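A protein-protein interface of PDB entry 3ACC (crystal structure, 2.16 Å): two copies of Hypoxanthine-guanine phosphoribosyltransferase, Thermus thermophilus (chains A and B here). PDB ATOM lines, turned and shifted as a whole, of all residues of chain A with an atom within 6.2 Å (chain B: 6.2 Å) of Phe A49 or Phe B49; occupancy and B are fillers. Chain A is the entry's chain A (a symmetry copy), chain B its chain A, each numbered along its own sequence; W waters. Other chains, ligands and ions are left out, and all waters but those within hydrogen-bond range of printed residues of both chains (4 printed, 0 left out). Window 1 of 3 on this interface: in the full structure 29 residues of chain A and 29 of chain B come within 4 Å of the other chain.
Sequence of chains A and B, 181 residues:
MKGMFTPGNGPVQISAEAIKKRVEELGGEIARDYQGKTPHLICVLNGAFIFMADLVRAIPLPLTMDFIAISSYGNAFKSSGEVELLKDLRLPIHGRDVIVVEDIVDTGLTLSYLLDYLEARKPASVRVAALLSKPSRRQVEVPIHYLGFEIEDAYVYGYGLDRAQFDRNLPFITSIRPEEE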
ATOM      1  N   CYS A  43      27.353  22.341  35.632  1.00  0.00           N
ATOM      2  CA  CYS A  43      27.548  22.345  34.183  1.00  0.00           C
ATOM      3  C   CYS A  43      28.694  21.420  33.774  1.00  0.00           C
ATOM      4  O   CYS A  43      29.793  21.494  34.333  1.00  0.00           O
ATOM      5  CB  CYS A  43      27.854  23.771  33.696  1.00  0.00           C
ATOM      6  SG  CYS A  43      28.286  23.916  31.922  1.00  0.00           S
ATOM      7  N   VAL A  44      28.437  20.551  32.799  1.00  0.00           N
ATOM      8  CA  VAL A  44      29.469  19.640  32.317  1.00  0.00           C
ATOM      9  C   VAL A  44      30.152  20.307  31.133  1.00  0.00           C
ATOM     10  O   VAL A  44      29.591  20.385  30.044  1.00  0.00           O
ATOM     11  CB  VAL A  44      28.874  18.273  31.879  1.00  0.00           C
ATOM     12  CG1 VAL A  44      29.982  17.344  31.398  1.00  0.00           C
ATOM     13  CG2 VAL A  44      28.145  17.619  33.050  1.00  0.00           C
ATOM     14  N   LEU A  45      31.361  20.810  31.362  1.00  0.00           N
ATOM     15  CA  LEU A  45      32.137  21.477  30.321  1.00  0.00           C
ATOM     16  C   LEU A  45      32.714  20.448  29.342  1.00  0.00           C
ATOM     17  O   LEU A  45      32.894  19.284  29.703  1.00  0.00           O
ATOM     18  CB  LEU A  45      33.273  22.291  30.958  1.00  0.00           C
ATOM     19  CG  LEU A  45      32.865  23.528  31.766  1.00  0.00           C
ATOM     20  CD1 LEU A  45      34.060  24.065  32.539  1.00  0.00           C
ATOM     21  CD2 LEU A  45      32.303  24.585  30.827  1.00  0.00           C
ATOM     22  N   ASN A  46      33.008  20.861  28.112  1.00  0.00           N
ATOM     23  CA  ASN A  46      32.822  22.234  27.644  1.00  0.00           C
ATOM     24  C   ASN A  46      31.515  22.433  26.878  1.00  0.00           C
ATOM     25  O   ASN A  46      30.979  23.540  26.817  1.00  0.00           O
ATOM     26  CB  ASN A  46      33.977  22.620  26.716  1.00  0.00           C
ATOM     27  CG  ASN A  46      35.307  22.740  27.438  1.00  0.00           C
ATOM     28  OD1 ASN A  46      36.355  22.873  26.803  1.00  0.00           O
ATOM     29  ND2 ASN A  46      35.273  22.700  28.763  1.00  0.00           N
ATOM     30  N   GLY A  47      31.009  21.352  26.296  1.00  0.00           N
ATOM     31  CA  GLY A  47      29.807  21.423  25.482  1.00  0.00           C
ATOM     32  C   GLY A  47      28.514  22.017  26.012  1.00  0.00           C
ATOM     33  O   GLY A  47      27.714  22.527  25.226  1.00  0.00           O
ATOM     34  N   ALA A  48      28.293  21.965  27.322  1.00  0.00           N
ATOM     35  CA  ALA A  48      27.044  22.476  27.883  1.00  0.00           C
ATOM     36  C   ALA A  48      27.043  23.908  28.404  1.00  0.00           C
ATOM     37  O   ALA A  48      26.023  24.362  28.922  1.00  0.00           O
ATOM     38  CB  ALA A  48      26.569  21.542  28.993  1.00  0.00           C
ATOM     39  N   PHE A  49      28.148  24.632  28.252  1.00  0.00           N
ATOM     40  CA  PHE A  49      28.214  25.987  28.792  1.00  0.00           C
ATOM     41  C   PHE A  49      27.236  27.013  28.201  1.00  0.00           C
ATOM     42  O   PHE A  49      26.867  27.964  28.888  1.00  0.00           O
ATOM     43  CB  PHE A  49      29.657  26.514  28.730  1.00  0.00           C
ATOM     44  CG  PHE A  49      29.995  27.257  27.469  1.00  0.00           C
ATOM     45  CD1 PHE A  49      29.944  28.647  27.435  1.00  0.00           C
ATOM     46  CD2 PHE A  49      30.401  26.573  26.332  1.00  0.00           C
ATOM     47  CE1 PHE A  49      30.303  29.345  26.281  1.00  0.00           C
ATOM     48  CE2 PHE A  49      30.762  27.263  25.174  1.00  0.00           C
ATOM     49  CZ  PHE A  49      30.713  28.651  25.152  1.00  0.00           C
ATOM     50  N   ILE A  50      26.818  26.837  26.949  1.00  0.00           N
ATOM     51  CA  ILE A  50      25.868  27.774  26.362  1.00  0.00           C
ATOM     52  C   ILE A  50      24.469  27.373  26.822  1.00  0.00           C
ATOM     53  O   ILE A  50      23.652  28.224  27.180  1.00  0.00           O
ATOM     54  CB  ILE A  50      25.941  27.789  24.812  1.00  0.00           C
ATOM     55  CG1 ILE A  50      27.311  28.327  24.368  1.00  0.00           C
ATOM     56  CG2 ILE A  50      24.813  28.657  24.247  1.00  0.00           C
ATOM     57  CD1 ILE A  50      27.444  28.590  22.877  1.00  0.00           C
ATOM     58  N   PHE A  51      24.193  26.072  26.816  1.00  0.00           N
ATOM     59  CA  PHE A  51      22.906  25.582  27.285  1.00  0.00           C
ATOM     60  C   PHE A  51      22.745  26.056  28.739  1.00  0.00           C
ATOM     61  O   PHE A  51      21.688  26.545  29.137  1.00  0.00           O
ATOM     62  CB  PHE A  51      22.872  24.047  27.199  1.00  0.00           C
ATOM     63  CG  PHE A  51      21.627  23.424  27.780  1.00  0.00           C
ATOM     64  CD1 PHE A  51      20.370  23.952  27.509  1.00  0.00           C
ATOM     65  CD2 PHE A  51      21.718  22.275  28.565  1.00  0.00           C
ATOM     66  CE1 PHE A  51      19.218  23.343  28.007  1.00  0.00           C
ATOM     67  CE2 PHE A  51      20.574  21.657  29.067  1.00  0.00           C
ATOM     68  CZ  PHE A  51      19.320  22.194  28.785  1.00  0.00           C
ATOM     69  N   MET A  52      23.815  25.930  29.517  1.00  0.00           N
ATOM     70  CA  MET A  52      23.823  26.355  30.916  1.00  0.00           C
ATOM     71  C   MET A  52      23.504  27.850  31.038  1.00  0.00           C
ATOM     72  O   MET A  52      22.655  28.249  31.837  1.00  0.00           O
ATOM     73  CB  MET A  52      25.198  26.085  31.530  1.00  0.00           C
ATOM     74  CG  MET A  52      25.344  26.509  32.985  1.00  0.00           C
ATOM     75  SD  MET A  52      24.603  25.322  34.118  1.00  0.00           S
ATOM     76  CE  MET A  52      25.249  25.901  35.702  1.00  0.00           C
ATOM     77  N   ALA A  53      24.191  28.667  30.242  1.00  0.00           N
ATOM     78  CA  ALA A  53      24.004  30.120  30.264  1.00  0.00           C
ATOM     79  C   ALA A  53      22.561  30.529  30.025  1.00  0.00           C
ATOM     80  O   ALA A  53      22.020  31.346  30.761  1.00  0.00           O
ATOM     81  CB  ALA A  53      24.906  30.787  29.232  1.00  0.00           C
ATOM     82  N   ASP A  54      21.937  29.966  28.995  1.00  0.00           N
ATOM     83  CA  ASP A  54      20.546  30.297  28.694  1.00  0.00           C
ATOM     84  C   ASP A  54      19.574  29.694  29.700  1.00  0.00           C
ATOM     85  O   ASP A  54      18.616  30.342  30.106  1.00  0.00           O
ATOM     86  CB  ASP A  54      20.172  29.827  27.286  1.00  0.00           C
ATOM     87  CG  ASP A  54      20.925  30.571  26.207  1.00  0.00           C
ATOM     88  OD1 ASP A  54      21.677  31.508  26.549  1.00  0.00           O
ATOM     89  OD2 ASP A  54      20.767  30.221  25.019  1.00  0.00           O
ATOM     90  N   VAL A  56      19.950  28.810  33.034  1.00  0.00           N
ATOM     91  CA  VAL A  56      19.922  29.457  34.341  1.00  0.00           C
ATOM     92  C   VAL A  56      19.176  30.789  34.332  1.00  0.00           C
ATOM     93  O   VAL A  56      18.538  31.160  35.320  1.00  0.00           O
ATOM     94  CB  VAL A  56      21.349  29.683  34.892  1.00  0.00           C
ATOM     95  CG1 VAL A  56      22.078  28.339  35.008  1.00  0.00           C
ATOM     96  CG2 VAL A  56      22.118  30.654  33.992  1.00  0.00           C
ATOM     97  N   MET A  65      25.976  27.408  41.362  1.00  0.00           N
ATOM     98  CA  MET A  65      26.440  26.574  40.271  1.00  0.00           C
ATOM     99  C   MET A  65      27.905  26.229  40.360  1.00  0.00           C
ATOM    100  O   MET A  65      28.654  26.832  41.123  1.00  0.00           O
ATOM    101  CB  MET A  65      26.127  27.230  38.917  1.00  0.00           C
ATOM    102  CG  MET A  65      25.925  28.738  38.940  1.00  0.00           C
ATOM    103  SD  MET A  65      25.467  29.411  37.306  1.00  0.00           S
ATOM    104  CE  MET A  65      23.913  30.208  37.659  1.00  0.00           C
ATOM    105  N   PHE A  67      31.209  24.037  37.818  1.00  0.00           N
ATOM    106  CA  PHE A  67      31.604  23.572  36.498  1.00  0.00           C
ATOM    107  C   PHE A  67      32.625  22.454  36.626  1.00  0.00           C
ATOM    108  O   PHE A  67      33.583  22.572  37.388  1.00  0.00           O
ATOM    109  CB  PHE A  67      32.222  24.733  35.716  1.00  0.00           C
ATOM    110  CG  PHE A  67      31.260  25.849  35.423  1.00  0.00           C
ATOM    111  CD1 PHE A  67      30.686  25.975  34.159  1.00  0.00           C
ATOM    112  CD2 PHE A  67      30.903  26.757  36.414  1.00  0.00           C
ATOM    113  CE1 PHE A  67      29.767  26.989  33.888  1.00  0.00           C
ATOM    114  CE2 PHE A  67      29.986  27.773  36.157  1.00  0.00           C
ATOM    115  CZ  PHE A  67      29.414  27.891  34.891  1.00  0.00           C
ATOM    116  N   TYR A 159      25.932  25.562  19.127  1.00  0.00           N
ATOM    117  CA  TYR A 159      25.324  25.891  20.414  1.00  0.00           C
ATOM    118  C   TYR A 159      26.133  25.302  21.582  1.00  0.00           C
ATOM    119  O   TYR A 159      25.570  24.730  22.526  1.00  0.00           O
ATOM    120  CB  TYR A 159      23.875  25.377  20.452  1.00  0.00           C
ATOM    121  CG  TYR A 159      23.032  25.945  21.580  1.00  0.00           C
ATOM    122  CD1 TYR A 159      22.574  27.264  21.543  1.00  0.00           C
ATOM    123  CD2 TYR A 159      22.711  25.172  22.691  1.00  0.00           C
ATOM    124  CE1 TYR A 159      21.806  27.799  22.594  1.00  0.00           C
ATOM    125  CE2 TYR A 159      21.956  25.694  23.749  1.00  0.00           C
ATOM    126  CZ  TYR A 159      21.508  27.007  23.696  1.00  0.00           C
ATOM    127  OH  TYR A 159      20.794  27.527  24.761  1.00  0.00           O
ATOM    128  N   GLY A 160      27.455  25.447  21.513  1.00  0.00           N
ATOM    129  CA  GLY A 160      28.316  24.927  22.562  1.00  0.00           C
ATOM    130  C   GLY A 160      29.016  23.625  22.196  1.00  0.00           C
ATOM    131  O   GLY A 160      30.137  23.373  22.641  1.00  0.00           O
ATOM    132  N   ARG A 168      31.575  25.757  18.075  1.00  0.00           N
ATOM    133  CA  ARG A 168      30.817  25.802  19.324  1.00  0.00           C
ATOM    134  C   ARG A 168      30.031  27.114  19.345  1.00  0.00           C
ATOM    135  O   ARG A 168      29.063  27.248  20.091  1.00  0.00           O
ATOM    136  CB  ARG A 168      31.738  25.785  20.551  1.00  0.00           C
ATOM    137  CG  ARG A 168      32.517  24.498  20.812  1.00  0.00           C
ATOM    138  CD  ARG A 168      33.304  24.665  22.119  1.00  0.00           C
ATOM    139  NE  ARG A 168      34.276  23.603  22.362  1.00  0.00           N
ATOM    140  CZ  ARG A 168      33.961  22.373  22.757  1.00  0.00           C
ATOM    141  NH1 ARG A 168      32.693  22.042  22.953  1.00  0.00           N
ATOM    142  NH2 ARG A 168      34.917  21.480  22.965  1.00  0.00           N
ATOM    143  N   CYS B  43      37.807  31.662  28.193  1.00  0.00           N
ATOM    144  CA  CYS B  43      36.849  32.149  29.186  1.00  0.00           C
ATOM    145  C   CYS B  43      37.391  31.988  30.605  1.00  0.00           C
ATOM    146  O   CYS B  43      37.856  30.907  30.984  1.00  0.00           O
ATOM    147  CB  CYS B  43      35.524  31.378  29.062  1.00  0.00           C
ATOM    148  SG  CYS B  43      34.275  31.759  30.347  1.00  0.00           S
ATOM    149  N   VAL B  44      37.330  33.062  31.390  1.00  0.00           N
ATOM    150  CA  VAL B  44      37.798  33.008  32.771  1.00  0.00           C
ATOM    151  C   VAL B  44      36.601  32.671  33.647  1.00  0.00           C
ATOM    152  O   VAL B  44      35.736  33.511  33.881  1.00  0.00           O
ATOM    153  CB  VAL B  44      38.417  34.359  33.223  1.00  0.00           C
ATOM    154  CG1 VAL B  44      38.908  34.260  34.662  1.00  0.00           C
ATOM    155  CG2 VAL B  44      39.590  34.728  32.318  1.00  0.00           C
ATOM    156  N   LEU B  45      36.546  31.426  34.109  1.00  0.00           N
ATOM    157  CA  LEU B  45      35.457  30.961  34.963  1.00  0.00           C
ATOM    158  C   LEU B  45      35.617  31.516  36.382  1.00  0.00           C
ATOM    159  O   LEU B  45      36.728  31.848  36.796  1.00  0.00           O
ATOM    160  CB  LEU B  45      35.442  29.425  34.998  1.00  0.00           C
ATOM    161  CG  LEU B  45      35.038  28.711  33.703  1.00  0.00           C
ATOM    162  CD1 LEU B  45      35.325  27.221  33.817  1.00  0.00           C
ATOM    163  CD2 LEU B  45      33.565  28.963  33.422  1.00  0.00           C
ATOM    164  N   ASN B  46      34.522  31.617  37.134  1.00  0.00           N
ATOM    165  CA  ASN B  46      33.186  31.223  36.690  1.00  0.00           C
ATOM    166  C   ASN B  46      32.356  32.399  36.176  1.00  0.00           C
ATOM    167  O   ASN B  46      31.444  32.224  35.369  1.00  0.00           O
ATOM    168  CB  ASN B  46      32.427  30.583  37.855  1.00  0.00           C
ATOM    169  CG  ASN B  46      32.998  29.240  38.272  1.00  0.00           C
ATOM    170  OD1 ASN B  46      32.607  28.684  39.299  1.00  0.00           O
ATOM    171  ND2 ASN B  46      33.918  28.710  37.478  1.00  0.00           N
ATOM    172  N   GLY B  47      32.682  33.595  36.650  1.00  0.00           N
ATOM    173  CA  GLY B  47      31.927  34.785  36.291  1.00  0.00           C
ATOM    174  C   GLY B  47      31.689  35.176  34.843  1.00  0.00           C
ATOM    175  O   GLY B  47      30.684  35.826  34.548  1.00  0.00           O
ATOM    176  N   ALA B  48      32.583  34.794  33.937  1.00  0.00           N
ATOM    177  CA  ALA B  48      32.432  35.184  32.537  1.00  0.00           C
ATOM    178  C   ALA B  48      31.743  34.195  31.604  1.00  0.00           C
ATOM    179  O   ALA B  48      31.634  34.468  30.408  1.00  0.00           O
ATOM    180  CB  ALA B  48      33.798  35.544  31.961  1.00  0.00           C
ATOM    181  N   PHE B  49      31.257  33.073  32.126  1.00  0.00           N
ATOM    182  CA  PHE B  49      30.647  32.068  31.260  1.00  0.00           C
ATOM    183  C   PHE B  49      29.379  32.488  30.505  1.00  0.00           C
ATOM    184  O   PHE B  49      29.105  31.951  29.433  1.00  0.00           O
ATOM    185  CB  PHE B  49      30.408  30.767  32.044  1.00  0.00           C
ATOM    186  CG  PHE B  49      29.060  30.674  32.699  1.00  0.00           C
ATOM    187  CD1 PHE B  49      28.021  29.984  32.081  1.00  0.00           C
ATOM    188  CD2 PHE B  49      28.840  31.238  33.948  1.00  0.00           C
ATOM    189  CE1 PHE B  49      26.781  29.854  32.706  1.00  0.00           C
ATOM    190  CE2 PHE B  49      27.602  31.112  34.580  1.00  0.00           C
ATOM    191  CZ  PHE B  49      26.574  30.417  33.957  1.00  0.00           C
ATOM    192  N   ILE B  50      28.606  33.429  31.044  1.00  0.00           N
ATOM    193  CA  ILE B  50      27.407  33.875  30.344  1.00  0.00           C
ATOM    194  C   ILE B  50      27.829  34.904  29.299  1.00  0.00           C
ATOM    195  O   ILE B  50      27.349  34.888  28.164  1.00  0.00           O
ATOM    196  CB  ILE B  50      26.358  34.488  31.309  1.00  0.00           C
ATOM    197  CG1 ILE B  50      25.843  33.400  32.265  1.00  0.00           C
ATOM    198  CG2 ILE B  50      25.202  35.089  30.505  1.00  0.00           C
ATOM    199  CD1 ILE B  50      24.662  33.811  33.128  1.00  0.00           C
ATOM    200  N   PHE B  51      28.735  35.800  29.681  1.00  0.00           N
ATOM    201  CA  PHE B  51      29.243  36.792  28.745  1.00  0.00           C
ATOM    202  C   PHE B  51      29.860  36.024  27.565  1.00  0.00           C
ATOM    203  O   PHE B  51      29.639  36.357  26.402  1.00  0.00           O
ATOM    204  CB  PHE B  51      30.293  37.672  29.441  1.00  0.00           C
ATOM    205  CG  PHE B  51      30.980  38.655  28.525  1.00  0.00           C
ATOM    206  CD1 PHE B  51      30.252  39.403  27.607  1.00  0.00           C
ATOM    207  CD2 PHE B  51      32.355  38.861  28.618  1.00  0.00           C
ATOM    208  CE1 PHE B  51      30.883  40.349  26.796  1.00  0.00           C
ATOM    209  CE2 PHE B  51      32.996  39.802  27.816  1.00  0.00           C
ATOM    210  CZ  PHE B  51      32.256  40.548  26.902  1.00  0.00           C
ATOM    211  N   MET B  52      30.615  34.976  27.881  1.00  0.00           N
ATOM    212  CA  MET B  52      31.253  34.136  26.868  1.00  0.00           C
ATOM    213  C   MET B  52      30.210  33.516  25.930  1.00  0.00           C
ATOM    214  O   MET B  52      30.351  33.572  24.707  1.00  0.00           O
ATOM    215  CB  MET B  52      32.041  33.014  27.550  1.00  0.00           C
ATOM    216  CG  MET B  52      32.735  32.049  26.598  1.00  0.00           C
ATOM    217  SD  MET B  52      34.266  32.728  25.939  1.00  0.00           S
ATOM    218  CE  MET B  52      35.000  31.261  25.181  1.00  0.00           C
ATOM    219  N   ALA B  53      29.167  32.928  26.514  1.00  0.00           N
ATOM    220  CA  ALA B  53      28.104  32.280  25.742  1.00  0.00           C
ATOM    221  C   ALA B  53      27.459  33.214  24.731  1.00  0.00           C
ATOM    222  O   ALA B  53      27.295  32.850  23.572  1.00  0.00           O
ATOM    223  CB  ALA B  53      27.037  31.719  26.676  1.00  0.00           C
ATOM    224  N   ASP B  54      27.091  34.414  25.166  1.00  0.00           N
ATOM    225  CA  ASP B  54      26.470  35.379  24.262  1.00  0.00           C
ATOM    226  C   ASP B  54      27.463  35.967  23.268  1.00  0.00           C
ATOM    227  O   ASP B  54      27.144  36.141  22.097  1.00  0.00           O
ATOM    228  CB  ASP B  54      25.811  36.513  25.052  1.00  0.00           C
ATOM    229  CG  ASP B  54      24.639  36.039  25.879  1.00  0.00           C
ATOM    230  OD1 ASP B  54      24.286  34.845  25.776  1.00  0.00           O
ATOM    231  OD2 ASP B  54      24.069  36.856  26.632  1.00  0.00           O
ATOM    232  N   VAL B  56      30.406  34.716  21.924  1.00  0.00           N
ATOM    233  CA  VAL B  56      30.816  33.823  20.845  1.00  0.00           C
ATOM    234  C   VAL B  56      29.747  33.660  19.767  1.00  0.00           C
ATOM    235  O   VAL B  56      30.065  33.494  18.587  1.00  0.00           O
ATOM    236  CB  VAL B  56      31.208  32.428  21.383  1.00  0.00           C
ATOM    237  CG1 VAL B  56      32.355  32.565  22.391  1.00  0.00           C
ATOM    238  CG2 VAL B  56      29.994  31.743  22.017  1.00  0.00           C
ATOM    239  N   MET B  65      37.824  27.470  21.649  1.00  0.00           N
ATOM    240  CA  MET B  65      37.753  28.051  22.975  1.00  0.00           C
ATOM    241  C   MET B  65      38.251  27.134  24.062  1.00  0.00           C
ATOM    242  O   MET B  65      38.424  25.937  23.852  1.00  0.00           O
ATOM    243  CB  MET B  65      36.320  28.518  23.284  1.00  0.00           C
ATOM    244  CG  MET B  65      35.216  27.850  22.478  1.00  0.00           C
ATOM    245  SD  MET B  65      33.565  28.534  22.848  1.00  0.00           S
ATOM    246  CE  MET B  65      33.026  29.084  21.241  1.00  0.00           C
ATOM    247  N   PHE B  67      38.547  27.009  28.762  1.00  0.00           N
ATOM    248  CA  PHE B  67      38.043  27.544  30.016  1.00  0.00           C
ATOM    249  C   PHE B  67      39.072  27.344  31.116  1.00  0.00           C
ATOM    250  O   PHE B  67      39.624  26.254  31.258  1.00  0.00           O
ATOM    251  CB  PHE B  67      36.750  26.817  30.394  1.00  0.00           C
ATOM    252  CG  PHE B  67      35.620  27.048  29.433  1.00  0.00           C
ATOM    253  CD1 PHE B  67      34.601  27.947  29.742  1.00  0.00           C
ATOM    254  CD2 PHE B  67      35.585  26.392  28.207  1.00  0.00           C
ATOM    255  CE1 PHE B  67      33.564  28.191  28.841  1.00  0.00           C
ATOM    256  CE2 PHE B  67      34.556  26.627  27.299  1.00  0.00           C
ATOM    257  CZ  PHE B  67      33.541  27.530  27.614  1.00  0.00           C
ATOM    258  N   TYR B 159      24.130  38.154  35.654  1.00  0.00           N
ATOM    259  CA  TYR B 159      24.684  37.859  34.334  1.00  0.00           C
ATOM    260  C   TYR B 159      26.005  37.078  34.441  1.00  0.00           C
ATOM    261  O   TYR B 159      26.985  37.382  33.749  1.00  0.00           O
ATOM    262  CB  TYR B 159      24.898  39.169  33.556  1.00  0.00           C
ATOM    263  CG  TYR B 159      25.139  38.987  32.068  1.00  0.00           C
ATOM    264  CD1 TYR B 159      24.098  38.633  31.206  1.00  0.00           C
ATOM    265  CD2 TYR B 159      26.410  39.149  31.526  1.00  0.00           C
ATOM    266  CE1 TYR B 159      24.322  38.447  29.830  1.00  0.00           C
ATOM    267  CE2 TYR B 159      26.650  38.959  30.159  1.00  0.00           C
ATOM    268  CZ  TYR B 159      25.604  38.607  29.317  1.00  0.00           C
ATOM    269  OH  TYR B 159      25.854  38.385  27.974  1.00  0.00           O
ATOM    270  N   GLY B 160      26.022  36.071  35.313  1.00  0.00           N
ATOM    271  CA  GLY B 160      27.220  35.268  35.497  1.00  0.00           C
ATOM    272  C   GLY B 160      28.006  35.613  36.755  1.00  0.00           C
ATOM    273  O   GLY B 160      28.634  34.741  37.357  1.00  0.00           O
ATOM    274  N   ARG B 168      24.003  34.412  40.009  1.00  0.00           N
ATOM    275  CA  ARG B 168      24.716  34.395  38.734  1.00  0.00           C
ATOM    276  C   ARG B 168      23.677  34.256  37.620  1.00  0.00           C
ATOM    277  O   ARG B 168      23.961  34.563  36.463  1.00  0.00           O
ATOM    278  CB  ARG B 168      25.676  33.202  38.634  1.00  0.00           C
ATOM    279  CG  ARG B 168      26.886  33.209  39.565  1.00  0.00           C
ATOM    280  CD  ARG B 168      27.749  31.980  39.247  1.00  0.00           C
ATOM    281  NE  ARG B 168      28.810  31.735  40.221  1.00  0.00           N
ATOM    282  CZ  ARG B 168      29.928  32.448  40.307  1.00  0.00           C
ATOM    283  NH1 ARG B 168      30.139  33.459  39.477  1.00  0.00           N
ATOM    284  NH2 ARG B 168      30.839  32.139  41.217  1.00  0.00           N
HETATM  285  O   HOH W   1      36.698  24.641  21.254  1.00  0.00           O
HETATM  286  O   HOH W   2      37.559  23.464  23.983  1.00  0.00           O
HETATM  287  O   HOH W   3      30.426  28.722  41.535  1.00  0.00           O
HETATM  288  O   HOH W   4      27.616  29.906  42.065  1.00  0.00           O
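N of Phe B49 sits at hydrogen-bond distance from SG of Cys B43.
The backbone NH of Phe A49 sits at hydrogen-bond distance from the side-chain sulfur of Cys A43, at 3.7 Å.
The backbone NH (N) of Gly B160 is in hydrogen-bond range of the backbone carbonyl oxygen (O) of Arg B168 (2.8 Å).
N of Gly A160 lies within hydrogen-bond range of O of Arg A168 (2.8 Å).
Among the printed residues, merely in contact across the chains: Ala A53 with Ala B53, Phe A49 with Phe B67, Phe A67 with Phe B49, Arg A168 with Met B65, Met A65 with Arg B168, Leu A45 with Leu B45, Phe A49 with Met B52, Met A52 with Phe B49, Met A65 with Phe B49, Phe A49 with Met B65, Phe A49 with Ala B53, Ala A53 with Phe B49, Asn A46 with Phe B67, Phe A67 with Asn B46 and Phe A49 with Phe B49.
Of chain B, only Phe B49, Met B52, Ala B53, Met B65 and Phe B67 come within 4 Å of Phe A49.
Of the printed residues of chain A, Leu B45 touches Leu A45 (3.6 Å).
Printed residues of chain A within 4 Å of Asn B46: Phe A67.
Of chain A, only Phe A49 (3.95 Å), Met A52 (3.7 Å), Ala A53 (3.7 Å), Met A65 (3.7 Å) and Phe A67 (3.5 Å) come within 4 Å of Phe B49.
Printed residues of chain A within 4 Å of Phe B67: Asn A46 and Phe A49.
The nearest residue of chain B that does not touch Phe A49 is Val B56 (4.5 Å).
The nearest residue of chain A that does not touch Phe B49 is Val A56 (4.5 Å).
Of the 18 printed residues of chain B, 8 touch a printed residue of chain A.
Leu A45 touches its own counterpart, Leu B45.
Asn A46 touches Phe B67, and with the chains exchanged Phe A67 touches Asn B46.
Phe A49 touches Met B65, and with the chains exchanged Met A65 touches Phe B49.
Ala A53 touches its own counterpart, Ala B53.
Water W2 lies within hydrogen-bond range of O of Met B65 (2.6 Å), OD1 of Asn A46 (3.1 Å) and NH2 of Arg A168 (3.5 Å).
Water W3 lies within hydrogen-bond range of the backbone carbonyl oxygen (O) of Met A65, the side-chain amide oxygen (OD1) of Asn B46 and the guanidinium group (NH2) of Arg B168.
Water W4 bridges NE of Arg B168 (2.9 Å) and N of Met A65 (3.1 Å).
Water W1 bridges the guanidinium group of Arg A168 (2.9 Å) and the backbone NH of Met B65 (3.1 Å).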
